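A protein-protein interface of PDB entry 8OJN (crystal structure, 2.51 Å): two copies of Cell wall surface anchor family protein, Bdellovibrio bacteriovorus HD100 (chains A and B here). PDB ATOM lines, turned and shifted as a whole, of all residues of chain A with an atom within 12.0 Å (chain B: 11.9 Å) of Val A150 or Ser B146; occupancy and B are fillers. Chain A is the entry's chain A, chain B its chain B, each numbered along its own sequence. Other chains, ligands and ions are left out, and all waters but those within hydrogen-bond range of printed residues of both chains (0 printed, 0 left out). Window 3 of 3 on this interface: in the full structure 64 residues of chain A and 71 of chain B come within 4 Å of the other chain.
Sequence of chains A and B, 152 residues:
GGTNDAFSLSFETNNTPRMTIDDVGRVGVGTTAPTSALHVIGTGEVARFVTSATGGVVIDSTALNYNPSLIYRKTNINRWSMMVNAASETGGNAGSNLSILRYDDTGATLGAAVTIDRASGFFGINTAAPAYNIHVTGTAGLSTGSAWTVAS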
ATOM      1  N   ILE A 134     -13.189  18.380   1.784  1.00  0.00           N
ATOM      2  CA  ILE A 134     -13.497  17.194   2.568  1.00  0.00           C
ATOM      3  C   ILE A 134     -12.845  16.011   1.869  1.00  0.00           C
ATOM      4  O   ILE A 134     -12.992  15.837   0.654  1.00  0.00           O
ATOM      5  CB  ILE A 134     -15.010  16.971   2.751  1.00  0.00           C
ATOM      6  CG1 ILE A 134     -15.251  15.651   3.483  1.00  0.00           C
ATOM      7  CG2 ILE A 134     -15.737  17.005   1.419  1.00  0.00           C
ATOM      8  CD1 ILE A 134     -16.654  15.498   4.009  1.00  0.00           C
ATOM      9  N   ALA A 140     -18.251   5.897   1.894  1.00  0.00           N
ATOM     10  CA  ALA A 140     -19.130   7.036   2.122  1.00  0.00           C
ATOM     11  C   ALA A 140     -20.578   6.579   2.033  1.00  0.00           C
ATOM     12  O   ALA A 140     -20.985   5.996   1.023  1.00  0.00           O
ATOM     13  CB  ALA A 140     -18.870   8.154   1.113  1.00  0.00           C
ATOM     14  N   GLY A 141     -21.349   6.842   3.085  1.00  0.00           N
ATOM     15  CA  GLY A 141     -22.741   6.437   3.116  1.00  0.00           C
ATOM     16  C   GLY A 141     -23.705   7.597   3.257  1.00  0.00           C
ATOM     17  O   GLY A 141     -23.573   8.415   4.173  1.00  0.00           O
ATOM     18  N   LEU A 142     -24.677   7.684   2.352  1.00  0.00           N
ATOM     19  CA  LEU A 142     -25.681   8.740   2.373  1.00  0.00           C
ATOM     20  C   LEU A 142     -27.060   8.102   2.347  1.00  0.00           C
ATOM     21  O   LEU A 142     -27.347   7.271   1.479  1.00  0.00           O
ATOM     22  CB  LEU A 142     -25.512   9.695   1.186  1.00  0.00           C
ATOM     23  CG  LEU A 142     -26.436  10.911   1.130  1.00  0.00           C
ATOM     24  CD1 LEU A 142     -26.256  11.779   2.356  1.00  0.00           C
ATOM     25  CD2 LEU A 142     -26.166  11.714  -0.126  1.00  0.00           C
ATOM     26  N   THR A 144     -29.928   9.464   1.629  1.00  0.00           N
ATOM     27  CA  THR A 144     -30.851  10.005   0.638  1.00  0.00           C
ATOM     28  C   THR A 144     -30.346   9.881  -0.799  1.00  0.00           C
ATOM     29  O   THR A 144     -30.773  10.654  -1.662  1.00  0.00           O
ATOM     30  CB  THR A 144     -31.159  11.473   0.938  1.00  0.00           C
ATOM     31  OG1 THR A 144     -29.933  12.202   1.059  1.00  0.00           O
ATOM     32  CG2 THR A 144     -31.952  11.601   2.224  1.00  0.00           C
ATOM     33  N   GLY A 145     -29.461   8.934  -1.087  1.00  0.00           N
ATOM     34  CA  GLY A 145     -29.073   8.766  -2.468  1.00  0.00           C
ATOM     35  C   GLY A 145     -27.577   8.628  -2.610  1.00  0.00           C
ATOM     36  O   GLY A 145     -26.852   8.423  -1.629  1.00  0.00           O
ATOM     37  N   SER A 146     -27.108   8.755  -3.851  1.00  0.00           N
ATOM     38  CA  SER A 146     -25.741   8.394  -4.195  1.00  0.00           C
ATOM     39  C   SER A 146     -24.864   9.568  -4.604  1.00  0.00           C
ATOM     40  O   SER A 146     -23.645   9.392  -4.717  1.00  0.00           O
ATOM     41  CB  SER A 146     -25.746   7.361  -5.327  1.00  0.00           C
ATOM     42  OG  SER A 146     -26.252   7.936  -6.518  1.00  0.00           O
ATOM     43  N   ALA A 147     -25.433  10.750  -4.829  1.00  0.00           N
ATOM     44  CA  ALA A 147     -24.668  11.891  -5.303  1.00  0.00           C
ATOM     45  C   ALA A 147     -24.850  13.085  -4.378  1.00  0.00           C
ATOM     46  O   ALA A 147     -25.873  13.211  -3.694  1.00  0.00           O
ATOM     47  CB  ALA A 147     -25.078  12.280  -6.725  1.00  0.00           C
ATOM     48  N   TRP A 148     -23.835  13.952  -4.357  1.00  0.00           N
ATOM     49  CA  TRP A 148     -23.982  15.267  -3.752  1.00  0.00           C
ATOM     50  C   TRP A 148     -25.003  16.082  -4.535  1.00  0.00           C
ATOM     51  O   TRP A 148     -25.111  15.972  -5.759  1.00  0.00           O
ATOM     52  CB  TRP A 148     -22.662  16.044  -3.751  1.00  0.00           C
ATOM     53  CG  TRP A 148     -21.484  15.486  -2.985  1.00  0.00           C
ATOM     54  CD1 TRP A 148     -20.543  14.614  -3.455  1.00  0.00           C
ATOM     55  CD2 TRP A 148     -21.075  15.830  -1.648  1.00  0.00           C
ATOM     56  NE1 TRP A 148     -19.598  14.367  -2.487  1.00  0.00           N
ATOM     57  CE2 TRP A 148     -19.901  15.100  -1.369  1.00  0.00           C
ATOM     58  CE3 TRP A 148     -21.599  16.666  -0.654  1.00  0.00           C
ATOM     59  CZ2 TRP A 148     -19.237  15.186  -0.138  1.00  0.00           C
ATOM     60  CZ3 TRP A 148     -20.938  16.744   0.571  1.00  0.00           C
ATOM     61  CH2 TRP A 148     -19.772  16.007   0.815  1.00  0.00           C
ATOM     62  N   THR A 149     -25.749  16.918  -3.822  1.00  0.00           N
ATOM     63  CA  THR A 149     -26.585  17.912  -4.477  1.00  0.00           C
ATOM     64  C   THR A 149     -25.727  19.116  -4.840  1.00  0.00           C
ATOM     65  O   THR A 149     -24.999  19.647  -3.994  1.00  0.00           O
ATOM     66  CB  THR A 149     -27.742  18.338  -3.573  1.00  0.00           C
ATOM     67  OG1 THR A 149     -28.693  17.271  -3.474  1.00  0.00           O
ATOM     68  CG2 THR A 149     -28.436  19.579  -4.137  1.00  0.00           C
ATOM     69  N   VAL A 150     -25.789  19.526  -6.106  1.00  0.00           N
ATOM     70  CA  VAL A 150     -25.037  20.685  -6.570  1.00  0.00           C
ATOM     71  C   VAL A 150     -25.551  21.910  -5.834  1.00  0.00           C
ATOM     72  O   VAL A 150     -26.660  22.388  -6.100  1.00  0.00           O
ATOM     73  CB  VAL A 150     -25.153  20.861  -8.096  1.00  0.00           C
ATOM     74  CG1 VAL A 150     -24.379  22.089  -8.556  1.00  0.00           C
ATOM     75  CG2 VAL A 150     -24.650  19.625  -8.806  1.00  0.00           C
ATOM     76  N   ALA A 151     -24.755  22.423  -4.905  1.00  0.00           N
ATOM     77  CA  ALA A 151     -25.160  23.574  -4.109  1.00  0.00           C
ATOM     78  C   ALA A 151     -24.940  24.861  -4.885  1.00  0.00           C
ATOM     79  O   ALA A 151     -23.965  25.570  -4.645  1.00  0.00           O
ATOM     80  CB  ALA A 151     -24.397  23.607  -2.794  1.00  0.00           C
ATOM     81  N   THR B 139     -29.306  14.919   3.836  1.00  0.00           N
ATOM     82  CA  THR B 139     -28.946  15.468   2.538  1.00  0.00           C
ATOM     83  C   THR B 139     -27.481  15.897   2.505  1.00  0.00           C
ATOM     84  O   THR B 139     -26.853  16.153   3.535  1.00  0.00           O
ATOM     85  CB  THR B 139     -29.844  16.657   2.201  1.00  0.00           C
ATOM     86  OG1 THR B 139     -29.639  17.691   3.167  1.00  0.00           O
ATOM     87  CG2 THR B 139     -31.294  16.236   2.248  1.00  0.00           C
ATOM     88  N   ALA B 140     -26.943  15.979   1.289  1.00  0.00           N
ATOM     89  CA  ALA B 140     -25.533  16.291   1.079  1.00  0.00           C
ATOM     90  C   ALA B 140     -25.412  17.298  -0.052  1.00  0.00           C
ATOM     91  O   ALA B 140     -25.822  17.009  -1.180  1.00  0.00           O
ATOM     92  CB  ALA B 140     -24.729  15.029   0.756  1.00  0.00           C
ATOM     93  N   GLY B 141     -24.856  18.464   0.247  1.00  0.00           N
ATOM     94  CA  GLY B 141     -24.619  19.491  -0.758  1.00  0.00           C
ATOM     95  C   GLY B 141     -23.132  19.719  -0.952  1.00  0.00           C
ATOM     96  O   GLY B 141     -22.371  19.766   0.020  1.00  0.00           O
ATOM     97  N   LEU B 142     -22.735  19.834  -2.224  1.00  0.00           N
ATOM     98  CA  LEU B 142     -21.326  20.088  -2.630  1.00  0.00           C
ATOM     99  C   LEU B 142     -21.308  21.288  -3.582  1.00  0.00           C
ATOM    100  O   LEU B 142     -22.031  21.252  -4.595  1.00  0.00           O
ATOM    101  CB  LEU B 142     -20.755  18.838  -3.305  1.00  0.00           C
ATOM    102  CG  LEU B 142     -19.314  18.967  -3.796  1.00  0.00           C
ATOM    103  CD1 LEU B 142     -18.391  19.381  -2.662  1.00  0.00           C
ATOM    104  CD2 LEU B 142     -18.834  17.669  -4.426  1.00  0.00           C
ATOM    105  N   SER B 143     -20.505  22.301  -3.254  1.00  0.00           N
ATOM    106  CA  SER B 143     -20.406  23.556  -4.044  1.00  0.00           C
ATOM    107  C   SER B 143     -19.866  23.321  -5.461  1.00  0.00           C
ATOM    108  O   SER B 143     -20.438  23.897  -6.403  1.00  0.00           O
ATOM    109  CB  SER B 143     -19.543  24.548  -3.307  1.00  0.00           C
ATOM    110  OG  SER B 143     -18.964  25.484  -4.202  1.00  0.00           O
ATOM    111  N   THR B 144     -18.837  22.482  -5.609  1.00  0.00           N
ATOM    112  CA  THR B 144     -18.172  22.299  -6.931  1.00  0.00           C
ATOM    113  C   THR B 144     -18.831  21.250  -7.839  1.00  0.00           C
ATOM    114  O   THR B 144     -18.470  21.233  -9.030  1.00  0.00           O
ATOM    115  CB  THR B 144     -16.669  22.051  -6.761  1.00  0.00           C
ATOM    116  OG1 THR B 144     -16.502  20.944  -5.875  1.00  0.00           O
ATOM    117  CG2 THR B 144     -15.936  23.257  -6.215  1.00  0.00           C
ATOM    118  N   GLY B 145     -19.744  20.412  -7.339  1.00  0.00           N
ATOM    119  CA  GLY B 145     -20.324  19.403  -8.249  1.00  0.00           C
ATOM    120  C   GLY B 145     -21.221  18.393  -7.555  1.00  0.00           C
ATOM    121  O   GLY B 145     -21.613  18.641  -6.401  1.00  0.00           O
ATOM    122  N   SER B 146     -21.508  17.276  -8.235  1.00  0.00           N
ATOM    123  CA  SER B 146     -22.382  16.251  -7.691  1.00  0.00           C
ATOM    124  C   SER B 146     -21.646  14.994  -7.253  1.00  0.00           C
ATOM    125  O   SER B 146     -22.275  14.099  -6.677  1.00  0.00           O
ATOM    126  CB  SER B 146     -23.446  15.867  -8.727  1.00  0.00           C
ATOM    127  OG  SER B 146     -22.892  14.987  -9.689  1.00  0.00           O
ATOM    128  N   ALA B 147     -20.342  14.902  -7.501  1.00  0.00           N
ATOM    129  CA  ALA B 147     -19.595  13.671  -7.305  1.00  0.00           C
ATOM    130  C   ALA B 147     -18.338  13.939  -6.497  1.00  0.00           C
ATOM    131  O   ALA B 147     -17.769  15.032  -6.543  1.00  0.00           O
ATOM    132  CB  ALA B 147     -19.206  13.031  -8.646  1.00  0.00           C
ATOM    133  N   TRP B 148     -17.918  12.922  -5.750  1.00  0.00           N
ATOM    134  CA  TRP B 148     -16.599  12.940  -5.144  1.00  0.00           C
ATOM    135  C   TRP B 148     -15.533  12.878  -6.227  1.00  0.00           C
ATOM    136  O   TRP B 148     -15.756  12.352  -7.321  1.00  0.00           O
ATOM    137  CB  TRP B 148     -16.412  11.748  -4.202  1.00  0.00           C
ATOM    138  CG  TRP B 148     -17.371  11.656  -3.048  1.00  0.00           C
ATOM    139  CD1 TRP B 148     -18.648  11.161  -3.073  1.00  0.00           C
ATOM    140  CD2 TRP B 148     -17.112  12.032  -1.687  1.00  0.00           C
ATOM    141  NE1 TRP B 148     -19.203  11.222  -1.812  1.00  0.00           N
ATOM    142  CE2 TRP B 148     -18.281  11.753  -0.945  1.00  0.00           C
ATOM    143  CE3 TRP B 148     -16.009  12.586  -1.027  1.00  0.00           C
ATOM    144  CZ2 TRP B 148     -18.375  12.008   0.424  1.00  0.00           C
ATOM    145  CZ3 TRP B 148     -16.108  12.842   0.330  1.00  0.00           C
ATOM    146  CH2 TRP B 148     -17.282  12.555   1.041  1.00  0.00           C
ATOM    147  N   THR B 149     -14.350  13.374  -5.888  1.00  0.00           N
ATOM    148  CA  THR B 149     -13.184  13.217  -6.785  1.00  0.00           C
ATOM    149  C   THR B 149     -12.468  11.969  -6.273  1.00  0.00           C
ATOM    150  O   THR B 149     -12.081  11.983  -5.106  1.00  0.00           O
ATOM    151  CB  THR B 149     -12.241  14.417  -6.702  1.00  0.00           C
ATOM    152  OG1 THR B 149     -12.892  15.528  -7.311  1.00  0.00           O
ATOM    153  CG2 THR B 149     -10.925  14.172  -7.399  1.00  0.00           C
ATOM    154  N   VAL B 150     -12.336  10.923  -7.087  1.00  0.00           N
ATOM    155  CA  VAL B 150     -11.655   9.711  -6.553  1.00  0.00           C
ATOM    156  C   VAL B 150     -10.230  10.121  -6.189  1.00  0.00           C
ATOM    157  O   VAL B 150      -9.538  10.667  -7.051  1.00  0.00           O
ATOM    158  CB  VAL B 150     -11.671   8.553  -7.566  1.00  0.00           C
ATOM    159  CG1 VAL B 150     -10.885   7.363  -7.048  1.00  0.00           C
ATOM    160  CG2 VAL B 150     -13.089   8.135  -7.904  1.00  0.00           C
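The backbone NH (N) of Thr A149 is in hydrogen-bond range of the backbone carbonyl oxygen (O) of Ala B140 (2.6 Å). N of Leu B142 sits at hydrogen-bond distance from O of Thr A149 (2.9 Å). The backbone carbonyl oxygen of Leu B142 lies within hydrogen-bond range of the backbone NH of Ala A151 (3.0 Å). N of Trp A148 lies within hydrogen-bond range of O of Ser B146, at 2.8 Å. NE1 of Trp A148 lies close to NE1 of Trp B148 (3.2 Å).
Ala A140 touches Trp B148. Ala B140 touches Leu A142 (CB to CD2, 3.7 Å). Thr B139 touches Thr A144 (CA to OG1, 3.7 Å). Ala A147 touches Ser B146. C of Trp A148 touches O of Ala B140 (3.6 Å). Gly B141 touches Trp A148. Leu B142 touches Trp A148 (CB to CB, 3.4 Å). O of Thr A149 touches CA of Gly B141, 3.3 Å away. Val A150 touches Leu B142 (CA to O, 3.6 Å). Val A150 touches Ser B146.
Ile A134 touches none of the printed residues of chain B. Printed residues of chain B within 4 Å of Leu A142: Ala B140. Of the printed residues of chain B, Thr A144 touches Thr B139. Of the printed residues of chain B, Ala A147 touches Ser B146 (3.3 Å). Of the printed residues of chain B, Trp A148 touches Ala B140 (3.6 Å), Gly B141 (3.3 Å), Leu B142 (3.4 Å), Gly B145 (3.9 Å), Ser B146 (2.8 Å), Ala B147 (3.8 Å) and Trp B148 (3.2 Å). Printed residues of chain B within 4 Å of Thr A149: Ala B140, Gly B141 and Leu B142. Val A150 touches just these residues of chain B: Leu B142, Gly B145 and Ser B146. Of the printed residues of chain B, Ala A151 touches Leu B142 (3.0 Å). Gly B141 touches just these residues of chain A: Trp A148 and Thr A149. No residue of chain A comes within 4 Å of Ser B143. Thr B144 touches none of the printed residues of chain A. Ser B146 touches just these residues of chain A: Ala A147, Trp A148 and Val A150. Ala B147 touches just one residue of chain A: Trp A148. Printed residues of chain A within 4 Å of Trp B148: Ala A140 (3.9 Å) and Trp A148 (3.2 Å).
Hydrophobic or aromatic side chains of chain A that line the printed part of chain B: Ala A140, Leu A142, Ala A147, Trp A148, Val A150 and Ala A151. Along chain A the printed residues that touch a printed residue of chain B span positions 140 to 151. Among the printed residues, no Asp or Glu carboxylate lies within 4 Å of a Lys or Arg side-chain nitrogen of the other chain.
Trp A148 touches Leu B142, but with the chains exchanged Leu A142 does not touch Trp B148 (7.2 Å). Trp A148 touches Ser B146, but with the chains exchanged Ser A146 does not touch Trp B148 (5.5 Å). Thr A149 touches Ala B140, but with the chains exchanged Ala A140 does not touch Thr B149 (9.8 Å). Val A150 touches Gly B145, but with the chains exchanged Gly A145 does not touch Val B150 (15.1 Å). Of the 18 pairs that touch across the chains among the printed residues, 3 have their exchanged pair printed and touching as well.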
